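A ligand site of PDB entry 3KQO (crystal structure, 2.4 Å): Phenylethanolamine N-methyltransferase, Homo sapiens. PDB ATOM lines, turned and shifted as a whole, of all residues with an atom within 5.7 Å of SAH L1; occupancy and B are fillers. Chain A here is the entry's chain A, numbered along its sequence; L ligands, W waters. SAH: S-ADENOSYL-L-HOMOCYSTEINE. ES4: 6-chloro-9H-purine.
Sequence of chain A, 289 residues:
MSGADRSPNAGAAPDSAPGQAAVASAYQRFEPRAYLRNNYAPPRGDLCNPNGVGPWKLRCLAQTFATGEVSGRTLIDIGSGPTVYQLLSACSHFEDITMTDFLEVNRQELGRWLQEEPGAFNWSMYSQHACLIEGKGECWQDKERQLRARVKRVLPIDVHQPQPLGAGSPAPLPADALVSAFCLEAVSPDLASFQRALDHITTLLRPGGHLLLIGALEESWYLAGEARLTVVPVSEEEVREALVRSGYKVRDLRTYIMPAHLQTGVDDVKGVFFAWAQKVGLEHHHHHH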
ATOM      1  N   TYR A  27      19.991  15.567  14.212  1.00  0.00           N
ATOM      2  CA  TYR A  27      19.632  15.644  15.623  1.00  0.00           C
ATOM      3  C   TYR A  27      20.663  16.416  16.438  1.00  0.00           C
ATOM      4  O   TYR A  27      20.474  16.620  17.636  1.00  0.00           O
ATOM      5  CB  TYR A  27      19.394  14.258  16.225  1.00  0.00           C
ATOM      6  CG  TYR A  27      17.967  13.805  16.079  1.00  0.00           C
ATOM      7  CD1 TYR A  27      17.603  12.930  15.064  1.00  0.00           C
ATOM      8  CD2 TYR A  27      16.971  14.300  16.922  1.00  0.00           C
ATOM      9  CE1 TYR A  27      16.288  12.527  14.915  1.00  0.00           C
ATOM     10  CE2 TYR A  27      15.651  13.902  16.779  1.00  0.00           C
ATOM     11  CZ  TYR A  27      15.312  13.025  15.771  1.00  0.00           C
ATOM     12  OH  TYR A  27      14.002  12.630  15.619  1.00  0.00           O
ATOM     13  N   PHE A  30      18.979  19.808  16.927  1.00  0.00           N
ATOM     14  CA  PHE A  30      17.711  19.707  17.647  1.00  0.00           C
ATOM     15  C   PHE A  30      17.704  20.616  18.882  1.00  0.00           C
ATOM     16  O   PHE A  30      18.495  20.413  19.799  1.00  0.00           O
ATOM     17  CB  PHE A  30      17.524  18.238  18.056  1.00  0.00           C
ATOM     18  CG  PHE A  30      16.279  17.972  18.849  1.00  0.00           C
ATOM     19  CD1 PHE A  30      15.184  17.368  18.258  1.00  0.00           C
ATOM     20  CD2 PHE A  30      16.220  18.283  20.206  1.00  0.00           C
ATOM     21  CE1 PHE A  30      14.037  17.099  18.985  1.00  0.00           C
ATOM     22  CE2 PHE A  30      15.080  18.011  20.940  1.00  0.00           C
ATOM     23  CZ  PHE A  30      13.995  17.422  20.333  1.00  0.00           C
ATOM     24  N   TYR A  35      11.310  22.400  20.454  1.00  0.00           N
ATOM     25  CA  TYR A  35      10.471  21.217  20.417  1.00  0.00           C
ATOM     26  C   TYR A  35       9.351  21.280  21.458  1.00  0.00           C
ATOM     27  O   TYR A  35       8.194  21.011  21.153  1.00  0.00           O
ATOM     28  CB  TYR A  35      11.318  19.961  20.597  1.00  0.00           C
ATOM     29  CG  TYR A  35      10.533  18.664  20.694  1.00  0.00           C
ATOM     30  CD1 TYR A  35      10.032  18.049  19.552  1.00  0.00           C
ATOM     31  CD2 TYR A  35      10.313  18.046  21.911  1.00  0.00           C
ATOM     32  CE1 TYR A  35       9.326  16.855  19.627  1.00  0.00           C
ATOM     33  CE2 TYR A  35       9.615  16.850  22.007  1.00  0.00           C
ATOM     34  CZ  TYR A  35       9.117  16.268  20.860  1.00  0.00           C
ATOM     35  OH  TYR A  35       8.424  15.081  20.954  1.00  0.00           O
ATOM     36  N   TYR A  40       4.219  21.050  23.246  1.00  0.00           N
ATOM     37  CA  TYR A  40       3.730  20.996  24.617  1.00  0.00           C
ATOM     38  C   TYR A  40       3.298  22.328  25.186  1.00  0.00           C
ATOM     39  O   TYR A  40       2.880  22.415  26.342  1.00  0.00           O
ATOM     40  CB  TYR A  40       4.746  20.279  25.498  1.00  0.00           C
ATOM     41  CG  TYR A  40       4.931  18.857  25.029  1.00  0.00           C
ATOM     42  CD1 TYR A  40       6.004  18.490  24.231  1.00  0.00           C
ATOM     43  CD2 TYR A  40       3.990  17.890  25.341  1.00  0.00           C
ATOM     44  CE1 TYR A  40       6.150  17.192  23.789  1.00  0.00           C
ATOM     45  CE2 TYR A  40       4.125  16.602  24.913  1.00  0.00           C
ATOM     46  CZ  TYR A  40       5.199  16.250  24.134  1.00  0.00           C
ATOM     47  OH  TYR A  40       5.329  14.953  23.708  1.00  0.00           O
ATOM     48  N   LYS A  57      -3.414  11.645  24.998  1.00  0.00           N
ATOM     49  CA  LYS A  57      -2.207  10.927  25.397  1.00  0.00           C
ATOM     50  C   LYS A  57      -2.212  10.538  26.870  1.00  0.00           C
ATOM     51  O   LYS A  57      -1.931   9.388  27.212  1.00  0.00           O
ATOM     52  CB  LYS A  57      -0.958  11.733  25.047  1.00  0.00           C
ATOM     53  CG  LYS A  57      -0.768  11.920  23.553  1.00  0.00           C
ATOM     54  CD  LYS A  57       0.687  12.140  23.158  1.00  0.00           C
ATOM     55  CE  LYS A  57       1.199  13.498  23.599  1.00  0.00           C
ATOM     56  NZ  LYS A  57       2.357  13.932  22.782  1.00  0.00           N
ATOM     57  N   ASP A  77      12.195   4.339  30.137  1.00  0.00           N
ATOM     58  CA  ASP A  77      11.541   5.198  29.168  1.00  0.00           C
ATOM     59  C   ASP A  77      12.522   5.463  28.039  1.00  0.00           C
ATOM     60  O   ASP A  77      13.624   5.953  28.266  1.00  0.00           O
ATOM     61  CB  ASP A  77      11.128   6.522  29.815  1.00  0.00           C
ATOM     62  CG  ASP A  77      10.419   7.441  28.862  1.00  0.00           C
ATOM     63  OD1 ASP A  77       9.605   6.942  28.046  1.00  0.00           O
ATOM     64  OD2 ASP A  77      10.650   8.659  28.932  1.00  0.00           O
ATOM     65  N   ILE A  78      12.107   5.112  26.814  1.00  0.00           N
ATOM     66  CA  ILE A  78      12.985   5.086  25.645  1.00  0.00           C
ATOM     67  C   ILE A  78      12.865   6.346  24.805  1.00  0.00           C
ATOM     68  O   ILE A  78      11.817   6.577  24.186  1.00  0.00           O
ATOM     69  CB  ILE A  78      12.638   3.899  24.726  1.00  0.00           C
ATOM     70  CG1 ILE A  78      12.668   2.573  25.497  1.00  0.00           C
ATOM     71  CG2 ILE A  78      13.569   3.879  23.508  1.00  0.00           C
ATOM     72  CD1 ILE A  78      14.067   2.113  25.869  1.00  0.00           C
ATOM     73  N   GLY A  79      13.922   7.139  24.746  1.00  0.00           N
ATOM     74  CA  GLY A  79      13.910   8.372  23.981  1.00  0.00           C
ATOM     75  C   GLY A  79      13.015   9.409  24.634  1.00  0.00           C
ATOM     76  O   GLY A  79      12.147  10.002  23.995  1.00  0.00           O
ATOM     77  N   SER A  80      13.235   9.632  25.924  1.00  0.00           N
ATOM     78  CA  SER A  80      12.447  10.548  26.715  1.00  0.00           C
ATOM     79  C   SER A  80      12.423  11.952  26.111  1.00  0.00           C
ATOM     80  O   SER A  80      11.467  12.695  26.297  1.00  0.00           O
ATOM     81  CB  SER A  80      13.012  10.644  28.130  1.00  0.00           C
ATOM     82  OG  SER A  80      13.222   9.354  28.686  1.00  0.00           O
ATOM     83  N   GLY A  81      13.478  12.302  25.387  1.00  0.00           N
ATOM     84  CA  GLY A  81      13.684  13.679  24.997  1.00  0.00           C
ATOM     85  C   GLY A  81      13.696  14.565  26.234  1.00  0.00           C
ATOM     86  O   GLY A  81      14.125  14.139  27.309  1.00  0.00           O
ATOM     87  N   PRO A  82      13.209  15.801  26.105  1.00  0.00           N
ATOM     88  CA  PRO A  82      13.123  16.715  27.245  1.00  0.00           C
ATOM     89  C   PRO A  82      11.740  16.697  27.904  1.00  0.00           C
ATOM     90  O   PRO A  82      11.337  17.710  28.454  1.00  0.00           O
ATOM     91  CB  PRO A  82      13.339  18.064  26.564  1.00  0.00           C
ATOM     92  CG  PRO A  82      12.502  17.903  25.297  1.00  0.00           C
ATOM     93  CD  PRO A  82      12.657  16.417  24.890  1.00  0.00           C
ATOM     94  N   THR A  83      11.023  15.577  27.847  1.00  0.00           N
ATOM     95  CA  THR A  83       9.645  15.552  28.371  1.00  0.00           C
ATOM     96  C   THR A  83       9.433  14.469  29.435  1.00  0.00           C
ATOM     97  O   THR A  83      10.091  13.430  29.405  1.00  0.00           O
ATOM     98  CB  THR A  83       8.590  15.388  27.252  1.00  0.00           C
ATOM     99  OG1 THR A  83       8.532  14.014  26.817  1.00  0.00           O
ATOM    100  CG2 THR A  83       8.912  16.295  26.062  1.00  0.00           C
ATOM    101  N   TYR A  85       5.906  13.960  30.826  1.00  0.00           N
ATOM    102  CA  TYR A  85       4.470  13.646  30.924  1.00  0.00           C
ATOM    103  C   TYR A  85       4.217  12.158  30.746  1.00  0.00           C
ATOM    104  O   TYR A  85       3.276  11.616  31.332  1.00  0.00           O
ATOM    105  CB  TYR A  85       3.678  14.387  29.840  1.00  0.00           C
ATOM    106  CG  TYR A  85       3.901  13.816  28.458  1.00  0.00           C
ATOM    107  CD1 TYR A  85       3.062  12.832  27.938  1.00  0.00           C
ATOM    108  CD2 TYR A  85       4.983  14.223  27.686  1.00  0.00           C
ATOM    109  CE1 TYR A  85       3.288  12.295  26.679  1.00  0.00           C
ATOM    110  CE2 TYR A  85       5.209  13.686  26.427  1.00  0.00           C
ATOM    111  CZ  TYR A  85       4.359  12.724  25.927  1.00  0.00           C
ATOM    112  OH  TYR A  85       4.587  12.203  24.687  1.00  0.00           O
ATOM    113  N   GLN A  86       5.045  11.500  29.941  1.00  0.00           N
ATOM    114  CA  GLN A  86       4.798  10.102  29.577  1.00  0.00           C
ATOM    115  C   GLN A  86       4.949   9.154  30.761  1.00  0.00           C
ATOM    116  O   GLN A  86       4.550   7.998  30.661  1.00  0.00           O
ATOM    117  CB  GLN A  86       5.676   9.656  28.392  1.00  0.00           C
ATOM    118  CG  GLN A  86       7.175   9.603  28.666  1.00  0.00           C
ATOM    119  CD  GLN A  86       7.891  10.907  28.337  1.00  0.00           C
ATOM    120  OE1 GLN A  86       7.301  11.988  28.361  1.00  0.00           O
ATOM    121  NE2 GLN A  86       9.179  10.813  28.010  1.00  0.00           N
ATOM    122  N   ASP A 101      17.837   9.453  26.682  1.00  0.00           N
ATOM    123  CA  ASP A 101      17.786  10.075  25.366  1.00  0.00           C
ATOM    124  C   ASP A 101      19.139  10.045  24.673  1.00  0.00           C
ATOM    125  O   ASP A 101      20.183   9.928  25.311  1.00  0.00           O
ATOM    126  CB  ASP A 101      17.263  11.512  25.417  1.00  0.00           C
ATOM    127  CG  ASP A 101      16.808  12.014  24.054  1.00  0.00           C
ATOM    128  OD1 ASP A 101      15.820  11.465  23.525  1.00  0.00           O
ATOM    129  OD2 ASP A 101      17.438  12.959  23.513  1.00  0.00           O
ATOM    130  N   PHE A 102      19.095  10.137  23.350  1.00  0.00           N
ATOM    131  CA  PHE A 102      20.307  10.159  22.539  1.00  0.00           C
ATOM    132  C   PHE A 102      21.103  11.437  22.796  1.00  0.00           C
ATOM    133  O   PHE A 102      22.316  11.403  22.948  1.00  0.00           O
ATOM    134  CB  PHE A 102      19.931  10.030  21.062  1.00  0.00           C
ATOM    135  CG  PHE A 102      21.111  10.013  20.138  1.00  0.00           C
ATOM    136  CD1 PHE A 102      21.935   8.907  20.054  1.00  0.00           C
ATOM    137  CD2 PHE A 102      21.375  11.103  19.328  1.00  0.00           C
ATOM    138  CE1 PHE A 102      23.023   8.889  19.203  1.00  0.00           C
ATOM    139  CE2 PHE A 102      22.461  11.093  18.454  1.00  0.00           C
ATOM    140  CZ  PHE A 102      23.288   9.992  18.397  1.00  0.00           C
ATOM    141  N   LEU A 103      20.397  12.574  22.865  1.00  0.00           N
ATOM    142  CA  LEU A 103      21.042  13.873  23.002  1.00  0.00           C
ATOM    143  C   LEU A 103      21.350  14.284  24.435  1.00  0.00           C
ATOM    144  O   LEU A 103      20.536  14.099  25.351  1.00  0.00           O
ATOM    145  CB  LEU A 103      20.194  14.961  22.344  1.00  0.00           C
ATOM    146  CG  LEU A 103      20.044  14.876  20.827  1.00  0.00           C
ATOM    147  CD1 LEU A 103      19.040  15.914  20.327  1.00  0.00           C
ATOM    148  CD2 LEU A 103      21.405  15.050  20.160  1.00  0.00           C
ATOM    149  N   ASN A 106      18.951  17.150  25.746  1.00  0.00           N
ATOM    150  CA  ASN A 106      17.704  16.634  26.304  1.00  0.00           C
ATOM    151  C   ASN A 106      17.871  16.053  27.697  1.00  0.00           C
ATOM    152  O   ASN A 106      16.996  16.203  28.554  1.00  0.00           O
ATOM    153  CB  ASN A 106      17.093  15.572  25.382  1.00  0.00           C
ATOM    154  CG  ASN A 106      16.326  16.176  24.223  1.00  0.00           C
ATOM    155  OD1 ASN A 106      16.079  15.505  23.219  1.00  0.00           O
ATOM    156  ND2 ASN A 106      15.967  17.447  24.358  1.00  0.00           N
ATOM    157  N   ILE A 157      21.379   6.814  25.188  1.00  0.00           N
ATOM    158  CA  ILE A 157      20.794   5.660  24.537  1.00  0.00           C
ATOM    159  C   ILE A 157      20.773   5.842  23.025  1.00  0.00           C
ATOM    160  O   ILE A 157      20.683   6.964  22.535  1.00  0.00           O
ATOM    161  CB  ILE A 157      19.364   5.402  25.050  1.00  0.00           C
ATOM    162  CG1 ILE A 157      18.851   4.055  24.543  1.00  0.00           C
ATOM    163  CG2 ILE A 157      18.432   6.543  24.635  1.00  0.00           C
ATOM    164  CD1 ILE A 157      17.428   3.752  24.976  1.00  0.00           C
ATOM    165  N   ASP A 158      20.869   4.732  22.301  1.00  0.00           N
ATOM    166  CA  ASP A 158      20.771   4.760  20.849  1.00  0.00           C
ATOM    167  C   ASP A 158      20.122   3.476  20.365  1.00  0.00           C
ATOM    168  O   ASP A 158      20.744   2.407  20.372  1.00  0.00           O
ATOM    169  CB  ASP A 158      22.145   4.928  20.196  1.00  0.00           C
ATOM    170  CG  ASP A 158      22.087   4.859  18.683  1.00  0.00           C
ATOM    171  OD1 ASP A 158      20.990   4.645  18.128  1.00  0.00           O
ATOM    172  OD2 ASP A 158      23.154   5.039  18.040  1.00  0.00           O
ATOM    173  N   VAL A 159      18.872   3.583  19.933  1.00  0.00           N
ATOM    174  CA  VAL A 159      18.082   2.410  19.567  1.00  0.00           C
ATOM    175  C   VAL A 159      18.625   1.727  18.309  1.00  0.00           C
ATOM    176  O   VAL A 159      18.314   0.565  18.037  1.00  0.00           O
ATOM    177  CB  VAL A 159      16.600   2.777  19.366  1.00  0.00           C
ATOM    178  CG1 VAL A 159      15.998   3.282  20.684  1.00  0.00           C
ATOM    179  CG2 VAL A 159      16.462   3.829  18.266  1.00  0.00           C
ATOM    180  N   HIS A 160      19.445   2.438  17.544  1.00  0.00           N
ATOM    181  CA  HIS A 160      20.029   1.849  16.341  1.00  0.00           C
ATOM    182  C   HIS A 160      21.111   0.830  16.702  1.00  0.00           C
ATOM    183  O   HIS A 160      21.591   0.101  15.845  1.00  0.00           O
ATOM    184  CB  HIS A 160      20.591   2.936  15.419  1.00  0.00           C
ATOM    185  CG  HIS A 160      19.564   3.894  14.925  1.00  0.00           C
ATOM    186  ND1 HIS A 160      18.378   3.480  14.350  1.00  0.00           N
ATOM    187  CD2 HIS A 160      19.528   5.245  14.912  1.00  0.00           C
ATOM    188  CE1 HIS A 160      17.661   4.541  14.016  1.00  0.00           C
ATOM    189  NE2 HIS A 160      18.341   5.630  14.339  1.00  0.00           N
ATOM    190  N   ALA A 181       7.754   7.165  23.614  1.00  0.00           N
ATOM    191  CA  ALA A 181       6.821   8.073  22.984  1.00  0.00           C
ATOM    192  C   ALA A 181       7.520   8.867  21.908  1.00  0.00           C
ATOM    193  O   ALA A 181       8.462   9.597  22.191  1.00  0.00           O
ATOM    194  CB  ALA A 181       6.213   9.014  24.029  1.00  0.00           C
ATOM    195  N   PHE A 182       7.035   8.699  20.676  1.00  0.00           N
ATOM    196  CA  PHE A 182       7.484   9.517  19.546  1.00  0.00           C
ATOM    197  C   PHE A 182       8.976   9.392  19.271  1.00  0.00           C
ATOM    198  O   PHE A 182       9.597  10.322  18.748  1.00  0.00           O
ATOM    199  CB  PHE A 182       7.093  10.967  19.763  1.00  0.00           C
ATOM    200  CG  PHE A 182       5.620  11.162  19.918  1.00  0.00           C
ATOM    201  CD1 PHE A 182       5.048  11.160  21.173  1.00  0.00           C
ATOM    202  CD2 PHE A 182       4.809  11.317  18.816  1.00  0.00           C
ATOM    203  CE1 PHE A 182       3.680  11.325  21.316  1.00  0.00           C
ATOM    204  CE2 PHE A 182       3.452  11.485  18.950  1.00  0.00           C
ATOM    205  CZ  PHE A 182       2.885  11.491  20.204  1.00  0.00           C
ATOM    206  N   CYS A 183       9.553   8.253  19.622  1.00  0.00           N
ATOM    207  CA  CYS A 183      10.976   8.056  19.372  1.00  0.00           C
ATOM    208  C   CYS A 183      11.243   7.274  18.081  1.00  0.00           C
ATOM    209  O   CYS A 183      11.731   7.846  17.093  1.00  0.00           O
ATOM    210  CB  CYS A 183      11.636   7.343  20.549  1.00  0.00           C
ATOM    211  SG  CYS A 183      13.400   7.082  20.308  1.00  0.00           S
ATOM    212  N   ALA A 186      10.551   8.522  14.695  1.00  0.00           N
ATOM    213  CA  ALA A 186      11.215   9.823  14.544  1.00  0.00           C
ATOM    214  C   ALA A 186      12.726   9.717  14.358  1.00  0.00           C
ATOM    215  O   ALA A 186      13.372  10.717  14.081  1.00  0.00           O
ATOM    216  CB  ALA A 186      10.905  10.711  15.757  1.00  0.00           C
ATOM    217  N   VAL A 187      13.284   8.517  14.533  1.00  0.00           N
ATOM    218  CA  VAL A 187      14.720   8.316  14.354  1.00  0.00           C
ATOM    219  C   VAL A 187      15.036   7.302  13.245  1.00  0.00           C
ATOM    220  O   VAL A 187      16.195   6.960  13.003  1.00  0.00           O
ATOM    221  CB  VAL A 187      15.402   7.831  15.667  1.00  0.00           C
ATOM    222  CG1 VAL A 187      15.093   8.787  16.806  1.00  0.00           C
ATOM    223  CG2 VAL A 187      14.938   6.425  16.019  1.00  0.00           C
ATOM    224  N   TYR A 222       9.435  16.869  10.990  1.00  0.00           N
ATOM    225  CA  TYR A 222       9.056  17.871  11.970  1.00  0.00           C
ATOM    226  C   TYR A 222      10.274  18.714  12.292  1.00  0.00           C
ATOM    227  O   TYR A 222      11.414  18.313  12.060  1.00  0.00           O
ATOM    228  CB  TYR A 222       8.500  17.219  13.235  1.00  0.00           C
ATOM    229  CG  TYR A 222       9.540  16.583  14.124  1.00  0.00           C
ATOM    230  CD1 TYR A 222      10.009  17.239  15.256  1.00  0.00           C
ATOM    231  CD2 TYR A 222      10.069  15.330  13.822  1.00  0.00           C
ATOM    232  CE1 TYR A 222      10.959  16.658  16.079  1.00  0.00           C
ATOM    233  CE2 TYR A 222      11.018  14.735  14.641  1.00  0.00           C
ATOM    234  CZ  TYR A 222      11.463  15.406  15.772  1.00  0.00           C
ATOM    235  OH  TYR A 222      12.404  14.852  16.585  1.00  0.00           O
HETATM  236  N   SAH L   1       9.591  11.167  24.427  1.00  0.00           N
HETATM  237  CA  SAH L   1       9.530  12.458  23.743  1.00  0.00           C
HETATM  238  CB  SAH L   1       9.932  12.260  22.275  1.00  0.00           C
HETATM  239  CG  SAH L   1      11.036  13.248  21.917  1.00  0.00           C
HETATM  240  SD  SAH L   1      11.178  13.341  20.104  1.00  0.00           S
HETATM  241  C   SAH L   1       8.065  12.922  23.778  1.00  0.00           C
HETATM  242  O   SAH L   1       7.219  12.137  24.040  1.00  0.00           O
HETATM  243  OXT SAH L   1       7.718  14.110  23.127  1.00  0.00           O
HETATM  244  C5' SAH L   1      12.256  12.022  19.499  1.00  0.00           C
HETATM  245  C4' SAH L   1      13.373  11.771  20.517  1.00  0.00           C
HETATM  246  O4' SAH L   1      14.219  10.669  20.043  1.00  0.00           O
HETATM  247  C3' SAH L   1      14.293  12.992  20.692  1.00  0.00           C
HETATM  248  O3' SAH L   1      14.452  13.280  22.064  1.00  0.00           O
HETATM  249  C2' SAH L   1      15.581  12.491  20.112  1.00  0.00           C
HETATM  250  O2' SAH L   1      16.748  13.144  20.523  1.00  0.00           O
HETATM  251  C1' SAH L   1      15.569  11.010  20.464  1.00  0.00           C
HETATM  252  N9  SAH L   1      16.533  10.342  19.614  1.00  0.00           N
HETATM  253  C8  SAH L   1      17.168  10.935  18.408  1.00  0.00           C
HETATM  254  N7  SAH L   1      18.039   9.914  17.826  1.00  0.00           N
HETATM  255  C5  SAH L   1      17.941   8.704  18.662  1.00  0.00           C
HETATM  256  C6  SAH L   1      18.602   7.358  18.542  1.00  0.00           C
HETATM  257  N6  SAH L   1      19.529   7.102  17.439  1.00  0.00           N
HETATM  258  N1  SAH L   1      18.310   6.334  19.532  1.00  0.00           N
HETATM  259  C2  SAH L   1      17.349   6.603  20.658  1.00  0.00           C
HETATM  260  N3  SAH L   1      16.705   7.937  20.771  1.00  0.00           N
HETATM  261  C4  SAH L   1      17.001   8.981  19.771  1.00  0.00           C
HETATM  262  C10 ES4 L   2       3.862  14.825  18.995  1.00  0.00           C
HETATM  263 CL01 ES4 L   2       1.142  15.164  19.256  1.00  0.00          CL
HETATM  264  C02 ES4 L   2       2.666  15.031  18.335  1.00  0.00           C
HETATM  265  N03 ES4 L   2       2.654  15.121  16.980  1.00  0.00           N
HETATM  266  C04 ES4 L   2       3.818  15.012  16.265  1.00  0.00           C
HETATM  267  N05 ES4 L   2       5.009  14.811  16.932  1.00  0.00           N
HETATM  268  C06 ES4 L   2       5.026  14.717  18.280  1.00  0.00           C
HETATM  269  N07 ES4 L   2       6.039  14.525  19.162  1.00  0.00           N
HETATM  270  C08 ES4 L   2       5.491  14.508  20.417  1.00  0.00           C
HETATM  271  N09 ES4 L   2       4.145  14.691  20.304  1.00  0.00           N
HETATM  272  O   HOH W   1      20.139   9.560  15.733  1.00  0.00           O
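OH of Tyr 40 lies close to OH of Tyr 85 (3.0 Å). The side-chain hydroxyl (OH) of Tyr 40 lies within hydrogen-bond range of the side-chain amino group (NZ) of Lys 57, at 3.3 Å. OD2 of Asp 101 sits close to OD1 of Asn 106 (2.9 Å). The backbone NH (N) of Gly 81 sits at hydrogen-bond distance from the side-chain carboxylate (OD1) of Asp 101 (3.1 Å). The backbone NH of Leu 103 sits at hydrogen-bond distance from the side-chain carboxylate of Asp 101, 3.1 Å away. The side-chain carboxylate (OD1) of Asp 158 sits at hydrogen-bond distance from the backbone NH (N) of His 160, at 2.8 Å. The backbone carbonyl oxygen (O) of Val 187 is in hydrogen-bond range of a ring nitrogen (NE2) of His 160, at 2.9 Å. NE2 of Gln 86 is in hydrogen-bond range of OD2 of Asp 77 (2.8 Å).
OXT of SAH L1 lies within hydrogen-bond range of OH of Tyr 35, 2.5 Å away. An oxygen (OXT) of SAH L1 lies within hydrogen-bond range of the side-chain hydroxyl (OH) of Tyr 40. An oxygen (O3') of SAH L1 sits at hydrogen-bond distance from the side-chain carboxylate of Asp 101 (2.7 Å). OH of Tyr 85 sits at hydrogen-bond distance from O of SAH L1. N of Val 159 is in hydrogen-bond range of N1 of SAH L1, at 2.8 Å. A nitrogen (N) of SAH L1 is in hydrogen-bond range of the backbone carbonyl oxygen of Gly 79. The side-chain carboxylate of Asp 158 lies within hydrogen-bond range of a nitrogen (N6) of SAH L1 (2.9 Å). N of SAH L1 sits at hydrogen-bond distance from O of Ala 181. The side-chain amide oxygen (OD1) of Asn 106 sits at hydrogen-bond distance from an oxygen (O3') of SAH L1, 3.0 Å away. The backbone carbonyl oxygen of Ser 80 lies within hydrogen-bond range of a nitrogen (N) of SAH L1, 3.1 Å away. SG of Cys 183 sits at hydrogen-bond distance from N3 of SAH L1, at 3.4 Å. The side-chain hydroxyl of Tyr 35 lies within hydrogen-bond range of a nitrogen (N07) of ES4 L2 (3.0 Å). A nitrogen (N09) of ES4 L2 is in hydrogen-bond range of the side-chain amino group of Lys 57 (3.1 Å).
A sulfur (SD) of SAH L1 lies close to the backbone carbonyl oxygen of Phe 182 (3.7 Å). Tyr 27 touches SAH L1. Gly 81 touches SAH L1. Thr 83 touches SAH L1. Gln 86 touches SAH L1. CB of Phe 102 touches C4 of SAH L1, 3.4 Å away. Leu 103 touches SAH L1 (CD1 to O2', 3.6 Å). Ile 157 touches SAH L1. CD2 of His 160 touches N6 of SAH L1, at 3.1 Å. Val 187 touches SAH L1. 21 residues have an atom within 4 Å of SAH L1: Tyr 27, Tyr 35, Tyr 40, Gly 79, Ser 80, Gly 81, Thr 83, Tyr 85, Gln 86, Asp 101, Phe 102, Leu 103, Asn 106, Ile 157, Asp 158, Val 159, His 160, Ala 181, Phe 182, Cys 183 and Val 187. The nearest printed residue that does not touch SAH L1 is Tyr 222 (4.02 Å).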
